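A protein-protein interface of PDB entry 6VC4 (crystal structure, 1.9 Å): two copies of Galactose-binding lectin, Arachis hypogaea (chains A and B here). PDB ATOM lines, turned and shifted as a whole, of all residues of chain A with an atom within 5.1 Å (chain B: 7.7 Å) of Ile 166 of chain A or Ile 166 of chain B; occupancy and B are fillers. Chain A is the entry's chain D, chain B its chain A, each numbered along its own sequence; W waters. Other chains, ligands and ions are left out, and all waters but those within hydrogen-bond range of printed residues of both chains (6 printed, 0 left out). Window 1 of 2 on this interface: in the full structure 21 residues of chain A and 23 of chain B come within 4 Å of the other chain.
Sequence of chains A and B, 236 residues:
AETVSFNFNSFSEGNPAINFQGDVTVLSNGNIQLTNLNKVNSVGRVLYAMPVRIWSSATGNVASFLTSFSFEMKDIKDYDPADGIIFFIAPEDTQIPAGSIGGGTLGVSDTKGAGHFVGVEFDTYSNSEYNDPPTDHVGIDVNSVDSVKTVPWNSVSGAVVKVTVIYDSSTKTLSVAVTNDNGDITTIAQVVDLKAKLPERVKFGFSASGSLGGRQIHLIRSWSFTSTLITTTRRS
The side-chain hydroxyl of Thr 187 of chain A is in hydrogen-bond range of the side-chain hydroxyl of Ser 64 of chain B, at 2.7 Å.
The side-chain carboxylate of Asp 168 of chain B is in hydrogen-bond range of the side-chain hydroxyl of Thr 187 of chain A, 2.6 Å away.
The side-chain hydroxyl of Thr 187 of chain B lies within hydrogen-bond range of the side-chain carboxylate of Asp 168 of chain A.
The backbone NH (N) of Ile 188 of chain B is in hydrogen-bond range of the side-chain carboxylate (OD1) of Asp 168 of chain A, at 3.4 Å.
OG of Ser 64 of chain B lies close to O of Tyr 167 of chain B (3.5 Å).
The backbone NH of Ser 169 of chain B lies within hydrogen-bond range of the side-chain hydroxyl of Ser 64 of chain B (3.0 Å).
N of Tyr 167 of chain B sits at hydrogen-bond distance from O of Phe 65 of chain B, at 2.9 Å.
N of Ser 175 of chain B sits at hydrogen-bond distance from O of Ile 166 of chain B (2.8 Å).
N of Ser 175 of chain A is in hydrogen-bond range of O of Ile 166 of chain A, 2.8 Å away.
N of Asp 168 of chain A sits at hydrogen-bond distance from O of Thr 173 of chain A (2.9 Å).
Among the printed residues, pairs that only touch across the chains: Phe 65 of chain A with Ile 185 of chain B, Thr 164 of chain A with Thr 164 of chain B, Thr 164 of chain A with Ile 166 of chain B, Ile 166 of chain A with Thr 164 of chain B, Ile 166 of chain A with Ile 166 of chain B, Ile 166 of chain A with Ser 175 of chain B, Ile 166 of chain A with Ala 177 of chain B, Asp 168 of chain A with Ala 189 of chain B, Thr 173 of chain A with Thr 173 of chain B, Ser 175 of chain A with Ile 166 of chain B and Thr 187 of chain A with Tyr 167 of chain B.
Printed residues of chain B within 4 Å of Phe 65 of chain A: Ile 185.
Of the printed residues of chain B, Thr 164 of chain A touches Thr 164 (3.8 Å) and Ile 166 (3.97 Å).
Ile 166 of chain A touches just these residues of chain B: Thr 164, Ile 166, Ser 175 and Ala 177.
Ile 166 of chain B touches just these residues of chain A: Thr 164, Ile 166 and Ser 175.
Of the printed residues of chain A, Asp 168 of chain B touches Thr 187.
Printed residues of chain A within 4 Å of Ala 177 of chain B: Ile 166 (3.9 Å).
Printed residues of chain A within 4 Å of Ala 189 of chain B: Asp 168.
The nearest printed residue of chain A that does not touch Ile 166 of chain B is Ala 177 of chain A (4.03 Å).
Hydrophobic or aromatic side chains of chain A that line the printed part of chain B: Ile 166.
Of the 25 printed residues of chain B, 12 touch a printed residue of chain A.
Among the printed residues, 15 pairs touch across the chains.
Among the printed residues, no Asp or Glu carboxylate lies within 4 Å of a Lys or Arg side-chain nitrogen of the other chain.
Thr 164 of chain A touches Ile 166 of chain B, and with the chains exchanged Ile 166 of chain A touches Thr 164 of chain B.
Ile 166 of chain A touches Ala 177 of chain B, but with the chains exchanged Ala 177 of chain A does not touch Ile 166 of chain B (4.03 Å).
Asp 168 of chain A touches Thr 187 of chain B, and with the chains exchanged Thr 187 of chain A touches Asp 168 of chain B.
Thr 173 of chain A touches its own counterpart, Thr 173 of chain B.
Water W5 lies within hydrogen-bond range of the side-chain hydroxyl of Ser 175 of chain A, the backbone carbonyl oxygen of Thr 173 of chain B and the backbone carbonyl oxygen of Ile 166 of chain B.
Water W3 lies within hydrogen-bond range of OG of Ser 175 of chain B (2.7 Å), O of Thr 173 of chain A (3.0 Å) and O of Ile 166 of chain A (3.3 Å).
Water W6 lies within hydrogen-bond range of OD1 of Asp 168 of chain B (2.9 Å), OG of Ser 169 of chain B (3.1 Å), OG1 of Thr 187 of chain A (3.3 Å) and OG of Ser 64 of chain B (3.5 Å).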
ATOM      1  N   PHE A  65       9.775  14.780  -2.350  1.00  0.00           N
ATOM      2  CA  PHE A  65       9.057  14.831  -3.612  1.00  0.00           C
ATOM      3  C   PHE A  65       7.610  14.420  -3.443  1.00  0.00           C
ATOM      4  O   PHE A  65       7.244  13.740  -2.486  1.00  0.00           O
ATOM      5  CB  PHE A  65       9.731  14.051  -4.762  1.00  0.00           C
ATOM      6  CG  PHE A  65       9.845  12.549  -4.633  1.00  0.00           C
ATOM      7  CD1 PHE A  65       8.756  11.727  -4.899  1.00  0.00           C
ATOM      8  CD2 PHE A  65      11.068  11.953  -4.334  1.00  0.00           C
ATOM      9  CE1 PHE A  65       8.869  10.340  -4.795  1.00  0.00           C
ATOM     10  CE2 PHE A  65      11.183  10.565  -4.264  1.00  0.00           C
ATOM     11  CZ  PHE A  65      10.078   9.773  -4.470  1.00  0.00           C
ATOM     12  N   LEU A  66       6.786  14.875  -4.379  1.00  0.00           N
ATOM     13  CA  LEU A  66       5.368  14.559  -4.486  1.00  0.00           C
ATOM     14  C   LEU A  66       5.114  14.201  -5.919  1.00  0.00           C
ATOM     15  O   LEU A  66       5.449  14.973  -6.816  1.00  0.00           O
ATOM     16  CB  LEU A  66       4.480  15.735  -4.017  1.00  0.00           C
ATOM     17  CG  LEU A  66       2.989  15.662  -4.402  1.00  0.00           C
ATOM     18  CD1 LEU A  66       2.250  14.602  -3.592  1.00  0.00           C
ATOM     19  CD2 LEU A  66       2.312  17.053  -4.217  1.00  0.00           C
ATOM     20  N   THR A 164      -0.650   8.339  -5.726  1.00  0.00           N
ATOM     21  CA  THR A 164      -0.039   9.519  -5.153  1.00  0.00           C
ATOM     22  C   THR A 164       1.103   9.009  -4.275  1.00  0.00           C
ATOM     23  O   THR A 164       0.911   8.095  -3.476  1.00  0.00           O
ATOM     24  CB  THR A 164      -1.050  10.409  -4.392  1.00  0.00           C
ATOM     25  OG1 THR A 164      -1.944  11.006  -5.321  1.00  0.00           O
ATOM     26  CG2 THR A 164      -0.355  11.535  -3.610  1.00  0.00           C
ATOM     27  N   VAL A 165       2.283   9.597  -4.441  1.00  0.00           N
ATOM     28  CA  VAL A 165       3.469   9.203  -3.690  1.00  0.00           C
ATOM     29  C   VAL A 165       4.081  10.435  -3.031  1.00  0.00           C
ATOM     30  O   VAL A 165       4.269  11.458  -3.681  1.00  0.00           O
ATOM     31  CB  VAL A 165       4.508   8.459  -4.573  1.00  0.00           C
ATOM     32  CG1 VAL A 165       5.732   8.014  -3.767  1.00  0.00           C
ATOM     33  CG2 VAL A 165       3.891   7.284  -5.331  1.00  0.00           C
ATOM     34  N   ILE A 166       4.418  10.319  -1.748  1.00  0.00           N
ATOM     35  CA  ILE A 166       5.111  11.370  -1.019  1.00  0.00           C
ATOM     36  C   ILE A 166       6.396  10.781  -0.463  1.00  0.00           C
ATOM     37  O   ILE A 166       6.352   9.802   0.272  1.00  0.00           O
ATOM     38  CB  ILE A 166       4.285  12.039   0.123  1.00  0.00           C
ATOM     39  CG1 ILE A 166       2.929  12.620  -0.383  1.00  0.00           C
ATOM     40  CG2 ILE A 166       5.131  13.105   0.881  1.00  0.00           C
ATOM     41  CD1 ILE A 166       1.945  13.015   0.729  1.00  0.00           C
ATOM     42  N   TYR A 167       7.518  11.440  -0.734  1.00  0.00           N
ATOM     43  CA  TYR A 167       8.769  11.101  -0.066  1.00  0.00           C
ATOM     44  C   TYR A 167       9.118  12.292   0.853  1.00  0.00           C
ATOM     45  O   TYR A 167       9.313  13.407   0.388  1.00  0.00           O
ATOM     46  CB  TYR A 167       9.908  10.733  -1.017  1.00  0.00           C
ATOM     47  CG  TYR A 167      11.140  10.320  -0.263  1.00  0.00           C
ATOM     48  CD1 TYR A 167      11.197   9.097   0.398  1.00  0.00           C
ATOM     49  CD2 TYR A 167      12.219  11.193  -0.115  1.00  0.00           C
ATOM     50  CE1 TYR A 167      12.318   8.729   1.143  1.00  0.00           C
ATOM     51  CE2 TYR A 167      13.359  10.821   0.604  1.00  0.00           C
ATOM     52  CZ  TYR A 167      13.407   9.583   1.217  1.00  0.00           C
ATOM     53  OH  TYR A 167      14.512   9.201   1.927  1.00  0.00           O
ATOM     54  N   ASP A 168       9.164  12.040   2.149  1.00  0.00           N
ATOM     55  CA  ASP A 168       9.510  13.044   3.151  1.00  0.00           C
ATOM     56  C   ASP A 168      10.985  12.826   3.527  1.00  0.00           C
ATOM     57  O   ASP A 168      11.301  11.824   4.176  1.00  0.00           O
ATOM     58  CB  ASP A 168       8.596  12.954   4.375  1.00  0.00           C
ATOM     59  CG  ASP A 168       9.029  13.939   5.440  1.00  0.00           C
ATOM     60  OD1 ASP A 168       8.997  15.148   5.166  1.00  0.00           O
ATOM     61  OD2 ASP A 168       9.550  13.497   6.482  1.00  0.00           O
ATOM     62  N   THR A 173      10.677   8.768   4.824  1.00  0.00           N
ATOM     63  CA  THR A 173       9.488   7.951   4.581  1.00  0.00           C
ATOM     64  C   THR A 173       8.962   8.101   3.172  1.00  0.00           C
ATOM     65  O   THR A 173       8.655   9.199   2.737  1.00  0.00           O
ATOM     66  CB  THR A 173       8.362   8.261   5.615  1.00  0.00           C
ATOM     67  OG1 THR A 173       8.898   8.090   6.926  1.00  0.00           O
ATOM     68  CG2 THR A 173       7.122   7.376   5.422  1.00  0.00           C
ATOM     69  N   LEU A 174       8.775   6.956   2.515  1.00  0.00           N
ATOM     70  CA  LEU A 174       8.117   6.812   1.211  1.00  0.00           C
ATOM     71  C   LEU A 174       6.658   6.348   1.466  1.00  0.00           C
ATOM     72  O   LEU A 174       6.456   5.254   1.981  1.00  0.00           O
ATOM     73  CB  LEU A 174       8.874   5.798   0.327  1.00  0.00           C
ATOM     74  CG  LEU A 174       8.428   5.695  -1.136  1.00  0.00           C
ATOM     75  CD1 LEU A 174       8.653   7.008  -1.903  1.00  0.00           C
ATOM     76  CD2 LEU A 174       9.122   4.558  -1.823  1.00  0.00           C
ATOM     77  N   SER A 175       5.660   7.185   1.147  1.00  0.00           N
ATOM     78  CA  SER A 175       4.255   6.863   1.360  1.00  0.00           C
ATOM     79  C   SER A 175       3.508   6.842   0.037  1.00  0.00           C
ATOM     80  O   SER A 175       3.673   7.730  -0.815  1.00  0.00           O
ATOM     81  CB  SER A 175       3.620   7.851   2.322  1.00  0.00           C
ATOM     82  OG  SER A 175       2.290   7.412   2.552  1.00  0.00           O
ATOM     83  N   VAL A 176       2.669   5.828  -0.122  1.00  0.00           N
ATOM     84  CA  VAL A 176       1.929   5.571  -1.350  1.00  0.00           C
ATOM     85  C   VAL A 176       0.440   5.421  -1.043  1.00  0.00           C
ATOM     86  O   VAL A 176       0.081   4.667  -0.152  1.00  0.00           O
ATOM     87  CB  VAL A 176       2.476   4.282  -2.038  1.00  0.00           C
ATOM     88  CG1 VAL A 176       1.839   4.049  -3.399  1.00  0.00           C
ATOM     89  CG2 VAL A 176       4.015   4.273  -2.140  1.00  0.00           C
ATOM     90  N   ALA A 177      -0.408   6.116  -1.800  1.00  0.00           N
ATOM     91  CA  ALA A 177      -1.879   5.985  -1.744  1.00  0.00           C
ATOM     92  C   ALA A 177      -2.355   5.626  -3.153  1.00  0.00           C
ATOM     93  O   ALA A 177      -2.024   6.322  -4.132  1.00  0.00           O
ATOM     94  CB  ALA A 177      -2.536   7.262  -1.237  1.00  0.00           C
ATOM     95  N   THR A 187      -3.052   1.889   0.959  1.00  0.00           N
ATOM     96  CA  THR A 187      -1.843   2.648   1.287  1.00  0.00           C
ATOM     97  C   THR A 187      -0.737   1.714   1.717  1.00  0.00           C
ATOM     98  O   THR A 187      -1.000   0.621   2.232  1.00  0.00           O
ATOM     99  CB  THR A 187      -2.049   3.718   2.388  1.00  0.00           C
ATOM    100  OG1 THR A 187      -2.346   3.074   3.629  1.00  0.00           O
ATOM    101  CG2 THR A 187      -3.073   4.769   2.032  1.00  0.00           C
ATOM    102  N   SER B  64      -7.075   3.906   6.589  1.00  0.00           N
ATOM    103  CA  SER B  64      -6.082   4.760   5.903  1.00  0.00           C
ATOM    104  C   SER B  64      -6.874   5.878   5.209  1.00  0.00           C
ATOM    105  O   SER B  64      -8.052   5.697   4.955  1.00  0.00           O
ATOM    106  CB  SER B  64      -5.239   4.001   4.896  1.00  0.00           C
ATOM    107  OG  SER B  64      -4.335   3.127   5.510  1.00  0.00           O
ATOM    108  N   PHE B  65      -6.261   7.026   4.996  1.00  0.00           N
ATOM    109  CA  PHE B  65      -6.979   8.054   4.218  1.00  0.00           C
ATOM    110  C   PHE B  65      -6.034   8.839   3.306  1.00  0.00           C
ATOM    111  O   PHE B  65      -4.852   8.926   3.567  1.00  0.00           O
ATOM    112  CB  PHE B  65      -7.878   8.923   5.094  1.00  0.00           C
ATOM    113  CG  PHE B  65      -7.171   9.818   6.070  1.00  0.00           C
ATOM    114  CD1 PHE B  65      -6.561  10.980   5.656  1.00  0.00           C
ATOM    115  CD2 PHE B  65      -7.136   9.516   7.415  1.00  0.00           C
ATOM    116  CE1 PHE B  65      -5.928  11.820   6.552  1.00  0.00           C
ATOM    117  CE2 PHE B  65      -6.487  10.351   8.305  1.00  0.00           C
ATOM    118  CZ  PHE B  65      -5.873  11.485   7.870  1.00  0.00           C
ATOM    119  N   LEU B  66      -6.611   9.315   2.214  1.00  0.00           N
ATOM    120  CA  LEU B  66      -5.958  10.219   1.253  1.00  0.00           C
ATOM    121  C   LEU B  66      -6.862  11.443   1.167  1.00  0.00           C
ATOM    122  O   LEU B  66      -8.036  11.295   0.928  1.00  0.00           O
ATOM    123  CB  LEU B  66      -5.813   9.558  -0.112  1.00  0.00           C
ATOM    124  CG  LEU B  66      -5.410  10.503  -1.234  1.00  0.00           C
ATOM    125  CD1 LEU B  66      -3.998  11.029  -1.020  1.00  0.00           C
ATOM    126  CD2 LEU B  66      -5.558   9.832  -2.581  1.00  0.00           C
ATOM    127  N   THR B  67      -6.285  12.603   1.379  1.00  0.00           N
ATOM    128  CA  THR B  67      -7.081  13.839   1.328  1.00  0.00           C
ATOM    129  C   THR B  67      -6.269  14.944   0.666  1.00  0.00           C
ATOM    130  O   THR B  67      -5.084  14.976   0.826  1.00  0.00           O
ATOM    131  CB  THR B  67      -7.648  14.194   2.703  1.00  0.00           C
ATOM    132  OG1 THR B  67      -8.578  15.246   2.529  1.00  0.00           O
ATOM    133  CG2 THR B  67      -6.610  14.578   3.725  1.00  0.00           C
ATOM    134  N   SER B  68      -6.956  15.759  -0.093  1.00  0.00           N
ATOM    135  CA  SER B  68      -6.361  16.902  -0.764  1.00  0.00           C
ATOM    136  C   SER B  68      -7.245  18.118  -0.590  1.00  0.00           C
ATOM    137  O   SER B  68      -8.470  18.006  -0.612  1.00  0.00           O
ATOM    138  CB  SER B  68      -6.125  16.615  -2.242  1.00  0.00           C
ATOM    139  OG  SER B  68      -5.040  15.721  -2.427  1.00  0.00           O
ATOM    140  N   VAL B 163      -2.503  21.130  -0.770  1.00  0.00           N
ATOM    141  CA  VAL B 163      -2.031  20.200   0.252  1.00  0.00           C
ATOM    142  C   VAL B 163      -2.527  18.784  -0.086  1.00  0.00           C
ATOM    143  O   VAL B 163      -3.663  18.614  -0.517  1.00  0.00           O
ATOM    144  CB  VAL B 163      -2.465  20.617   1.689  1.00  0.00           C
ATOM    145  CG1 VAL B 163      -1.893  19.658   2.749  1.00  0.00           C
ATOM    146  CG2 VAL B 163      -2.070  22.064   2.004  1.00  0.00           C
ATOM    147  N   THR B 164      -1.684  17.796   0.156  1.00  0.00           N
ATOM    148  CA  THR B 164      -1.995  16.388   0.012  1.00  0.00           C
ATOM    149  C   THR B 164      -1.564  15.722   1.309  1.00  0.00           C
ATOM    150  O   THR B 164      -0.440  15.927   1.780  1.00  0.00           O
ATOM    151  CB  THR B 164      -1.361  15.772  -1.250  1.00  0.00           C
ATOM    152  OG1 THR B 164      -2.004  16.313  -2.405  1.00  0.00           O
ATOM    153  CG2 THR B 164      -1.522  14.265  -1.288  1.00  0.00           C
ATOM    154  N   VAL B 165      -2.471  14.942   1.892  1.00  0.00           N
ATOM    155  CA  VAL B 165      -2.206  14.221   3.128  1.00  0.00           C
ATOM    156  C   VAL B 165      -2.475  12.730   2.929  1.00  0.00           C
ATOM    157  O   VAL B 165      -3.500  12.337   2.370  1.00  0.00           O
ATOM    158  CB  VAL B 165      -3.024  14.782   4.320  1.00  0.00           C
ATOM    159  CG1 VAL B 165      -2.683  14.056   5.612  1.00  0.00           C
ATOM    160  CG2 VAL B 165      -2.862  16.302   4.477  1.00  0.00           C
ATOM    161  N   ILE B 166      -1.527  11.895   3.382  1.00  0.00           N
ATOM    162  CA  ILE B 166      -1.695  10.458   3.372  1.00  0.00           C
ATOM    163  C   ILE B 166      -1.555   9.959   4.793  1.00  0.00           C
ATOM    164  O   ILE B 166      -0.524  10.212   5.430  1.00  0.00           O
ATOM    165  CB  ILE B 166      -0.720   9.691   2.433  1.00  0.00           C
ATOM    166  CG1 ILE B 166      -0.815  10.170   0.953  1.00  0.00           C
ATOM    167  CG2 ILE B 166      -0.946   8.155   2.556  1.00  0.00           C
ATOM    168  CD1 ILE B 166       0.374   9.755   0.094  1.00  0.00           C
ATOM    169  N   TYR B 167      -2.558   9.202   5.267  1.00  0.00           N
ATOM    170  CA  TYR B 167      -2.427   8.490   6.535  1.00  0.00           C
ATOM    171  C   TYR B 167      -2.372   7.001   6.217  1.00  0.00           C
ATOM    172  O   TYR B 167      -3.302   6.459   5.620  1.00  0.00           O
ATOM    173  CB  TYR B 167      -3.515   8.819   7.555  1.00  0.00           C
ATOM    174  CG  TYR B 167      -3.270   8.132   8.883  1.00  0.00           C
ATOM    175  CD1 TYR B 167      -2.233   8.543   9.724  1.00  0.00           C
ATOM    176  CD2 TYR B 167      -3.996   6.995   9.246  1.00  0.00           C
ATOM    177  CE1 TYR B 167      -1.951   7.865  10.908  1.00  0.00           C
ATOM    178  CE2 TYR B 167      -3.739   6.325  10.439  1.00  0.00           C
ATOM    179  CZ  TYR B 167      -2.734   6.780  11.281  1.00  0.00           C
ATOM    180  OH  TYR B 167      -2.481   6.125  12.464  1.00  0.00           O
ATOM    181  N   ASP B 168      -1.246   6.373   6.523  1.00  0.00           N
ATOM    182  CA  ASP B 168      -1.044   4.943   6.311  1.00  0.00           C
ATOM    183  C   ASP B 168      -1.278   4.244   7.646  1.00  0.00           C
ATOM    184  O   ASP B 168      -0.477   4.402   8.571  1.00  0.00           O
ATOM    185  CB  ASP B 168       0.360   4.643   5.763  1.00  0.00           C
ATOM    186  CG  ASP B 168       0.606   3.147   5.644  1.00  0.00           C
ATOM    187  OD1 ASP B 168      -0.088   2.495   4.856  1.00  0.00           O
ATOM    188  OD2 ASP B 168       1.422   2.621   6.407  1.00  0.00           O
ATOM    189  N   SER B 169      -2.395   3.505   7.765  1.00  0.00           N
ATOM    190  CA  SER B 169      -2.787   2.876   9.029  1.00  0.00           C
ATOM    191  C   SER B 169      -1.759   1.860   9.574  1.00  0.00           C
ATOM    192  O   SER B 169      -1.523   1.882  10.767  1.00  0.00           O
ATOM    193  CB  SER B 169      -4.154   2.219   8.901  1.00  0.00           C
ATOM    194  OG  SER B 169      -4.148   1.084   8.051  1.00  0.00           O
ATOM    195  N   LYS B 172       1.201   3.824  10.829  1.00  0.00           N
ATOM    196  CA  LYS B 172       0.618   4.926  11.618  1.00  0.00           C
ATOM    197  C   LYS B 172       1.260   6.263  11.183  1.00  0.00           C
ATOM    198  O   LYS B 172       1.337   7.213  11.959  1.00  0.00           O
ATOM    199  CB  LYS B 172       0.751   4.683  13.151  1.00  0.00           C
ATOM    200  CG  LYS B 172      -0.023   3.460  13.635  1.00  0.00           C
ATOM    201  CD  LYS B 172       0.377   3.009  15.040  1.00  0.00           C
ATOM    202  CE  LYS B 172      -0.394   1.771  15.456  1.00  0.00           C
ATOM    203  NZ  LYS B 172       0.078   0.539  14.763  1.00  0.00           N
ATOM    204  N   THR B 173       1.705   6.343   9.922  1.00  0.00           N
ATOM    205  CA  THR B 173       2.361   7.549   9.430  1.00  0.00           C
ATOM    206  C   THR B 173       1.379   8.522   8.791  1.00  0.00           C
ATOM    207  O   THR B 173       0.619   8.159   7.905  1.00  0.00           O
ATOM    208  CB  THR B 173       3.510   7.200   8.437  1.00  0.00           C
ATOM    209  OG1 THR B 173       4.427   6.298   9.090  1.00  0.00           O
ATOM    210  CG2 THR B 173       4.267   8.445   7.964  1.00  0.00           C
ATOM    211  N   LEU B 174       1.424   9.763   9.267  1.00  0.00           N
ATOM    212  CA  LEU B 174       0.720  10.911   8.706  1.00  0.00           C
ATOM    213  C   LEU B 174       1.753  11.678   7.843  1.00  0.00           C
ATOM    214  O   LEU B 174       2.701  12.235   8.394  1.00  0.00           O
ATOM    215  CB  LEU B 174       0.131  11.801   9.842  1.00  0.00           C
ATOM    216  CG  LEU B 174      -0.785  12.946   9.404  1.00  0.00           C
ATOM    217  CD1 LEU B 174      -2.052  12.406   8.719  1.00  0.00           C
ATOM    218  CD2 LEU B 174      -1.138  13.837  10.571  1.00  0.00           C
ATOM    219  N   SER B 175       1.626  11.623   6.507  1.00  0.00           N
ATOM    220  CA  SER B 175       2.530  12.335   5.596  1.00  0.00           C
ATOM    221  C   SER B 175       1.815  13.475   4.884  1.00  0.00           C
ATOM    222  O   SER B 175       0.686  13.303   4.420  1.00  0.00           O
ATOM    223  CB  SER B 175       3.150  11.379   4.578  1.00  0.00           C
ATOM    224  OG  SER B 175       4.093  12.118   3.818  1.00  0.00           O
ATOM    225  N   VAL B 176       2.471  14.648   4.838  1.00  0.00           N
ATOM    226  CA  VAL B 176       1.915  15.903   4.302  1.00  0.00           C
ATOM    227  C   VAL B 176       2.858  16.479   3.242  1.00  0.00           C
ATOM    228  O   VAL B 176       4.056  16.629   3.502  1.00  0.00           O
ATOM    229  CB  VAL B 176       1.671  16.966   5.450  1.00  0.00           C
ATOM    230  CG1 VAL B 176       0.962  18.209   4.931  1.00  0.00           C
ATOM    231  CG2 VAL B 176       0.923  16.368   6.637  1.00  0.00           C
ATOM    232  N   ALA B 177       2.297  16.849   2.079  1.00  0.00           N
ATOM    233  CA  ALA B 177       3.021  17.534   1.010  1.00  0.00           C
ATOM    234  C   ALA B 177       2.264  18.827   0.706  1.00  0.00           C
ATOM    235  O   ALA B 177       1.056  18.795   0.426  1.00  0.00           O
ATOM    236  CB  ALA B 177       3.157  16.644  -0.241  1.00  0.00           C
ATOM    237  N   VAL B 178       2.965  19.954   0.797  1.00  0.00           N
ATOM    238  CA  VAL B 178       2.408  21.298   0.608  1.00  0.00           C
ATOM    239  C   VAL B 178       3.054  21.934  -0.628  1.00  0.00           C
ATOM    240  O   VAL B 178       4.274  22.125  -0.650  1.00  0.00           O
ATOM    241  CB  VAL B 178       2.594  22.186   1.877  1.00  0.00           C
ATOM    242  CG1 VAL B 178       1.889  23.527   1.723  1.00  0.00           C
ATOM    243  CG2 VAL B 178       2.133  21.470   3.146  1.00  0.00           C
ATOM    244  N   ILE B 185       7.981  22.411  -3.120  1.00  0.00           N
ATOM    245  CA  ILE B 185       7.197  21.549  -2.250  1.00  0.00           C
ATOM    246  C   ILE B 185       7.803  21.553  -0.857  1.00  0.00           C
ATOM    247  O   ILE B 185       9.018  21.658  -0.709  1.00  0.00           O
ATOM    248  CB  ILE B 185       6.946  20.105  -2.764  1.00  0.00           C
ATOM    249  CG1 ILE B 185       8.234  19.388  -3.190  1.00  0.00           C
ATOM    250  CG2 ILE B 185       5.880  20.062  -3.839  1.00  0.00           C
ATOM    251  CD1 ILE B 185       8.466  18.258  -2.341  1.00  0.00           C
ATOM    252  N   THR B 186       6.938  21.470   0.161  1.00  0.00           N
ATOM    253  CA  THR B 186       7.302  21.378   1.579  1.00  0.00           C
ATOM    254  C   THR B 186       6.680  20.085   2.101  1.00  0.00           C
ATOM    255  O   THR B 186       5.497  19.857   1.864  1.00  0.00           O
ATOM    256  CB  THR B 186       6.816  22.627   2.350  1.00  0.00           C
ATOM    257  OG1 THR B 186       7.329  23.800   1.719  1.00  0.00           O
ATOM    258  CG2 THR B 186       7.231  22.614   3.828  1.00  0.00           C
ATOM    259  N   THR B 187       7.441  19.249   2.805  1.00  0.00           N
ATOM    260  CA  THR B 187       6.857  18.028   3.353  1.00  0.00           C
ATOM    261  C   THR B 187       7.098  17.925   4.841  1.00  0.00           C
ATOM    262  O   THR B 187       8.110  18.426   5.358  1.00  0.00           O
ATOM    263  CB  THR B 187       7.365  16.733   2.656  1.00  0.00           C
ATOM    264  OG1 THR B 187       8.753  16.530   2.947  1.00  0.00           O
ATOM    265  CG2 THR B 187       7.081  16.697   1.160  1.00  0.00           C
ATOM    266  N   ILE B 188       6.227  17.168   5.515  1.00  0.00           N
ATOM    267  CA  ILE B 188       6.365  16.880   6.947  1.00  0.00           C
ATOM    268  C   ILE B 188       5.627  15.575   7.217  1.00  0.00           C
ATOM    269  O   ILE B 188       4.534  15.367   6.703  1.00  0.00           O
ATOM    270  CB  ILE B 188       5.916  18.051   7.881  1.00  0.00           C
ATOM    271  CG1 ILE B 188       6.327  17.750   9.350  1.00  0.00           C
ATOM    272  CG2 ILE B 188       4.407  18.413   7.699  1.00  0.00           C
ATOM    273  CD1 ILE B 188       6.075  18.901  10.377  1.00  0.00           C
ATOM    274  N   ALA B 189       6.247  14.676   7.982  1.00  0.00           N
ATOM    275  CA  ALA B 189       5.652  13.367   8.276  1.00  0.00           C
ATOM    276  C   ALA B 189       5.882  13.010   9.740  1.00  0.00           C
ATOM    277  O   ALA B 189       6.893  13.387  10.309  1.00  0.00           O
ATOM    278  CB  ALA B 189       6.230  12.275   7.341  1.00  0.00           C
ATOM    279  N   GLN B 190       4.918  12.341  10.364  1.00  0.00           N
ATOM    280  CA  GLN B 190       5.017  11.969  11.781  1.00  0.00           C
ATOM    281  C   GLN B 190       4.220  10.717  12.037  1.00  0.00           C
ATOM    282  O   GLN B 190       3.100  10.595  11.555  1.00  0.00           O
ATOM    283  CB  GLN B 190       4.486  13.136  12.670  1.00  0.00           C
ATOM    284  CG  GLN B 190       4.444  12.894  14.202  1.00  0.00           C
ATOM    285  CD  GLN B 190       5.808  12.623  14.759  1.00  0.00           C
ATOM    286  OE1 GLN B 190       6.758  13.370  14.499  1.00  0.00           O
ATOM    287  NE2 GLN B 190       5.948  11.546  15.516  1.00  0.00           N
HETATM  288  O   HOH W   1       7.525   6.901   9.178  1.00  0.00           O
HETATM  289  O   HOH W   2       9.088  15.256   8.539  1.00  0.00           O
HETATM  290  O   HOH W   3       6.008  10.263   3.514  1.00  0.00           O
HETATM  291  O   HOH W   4      -3.910  13.145  -4.508  1.00  0.00           O
HETATM  292  O   HOH W   5       1.908   8.035   5.125  1.00  0.00           O
HETATM  293  O   HOH W   6      -1.977   0.584   5.839  1.00  0.00           O
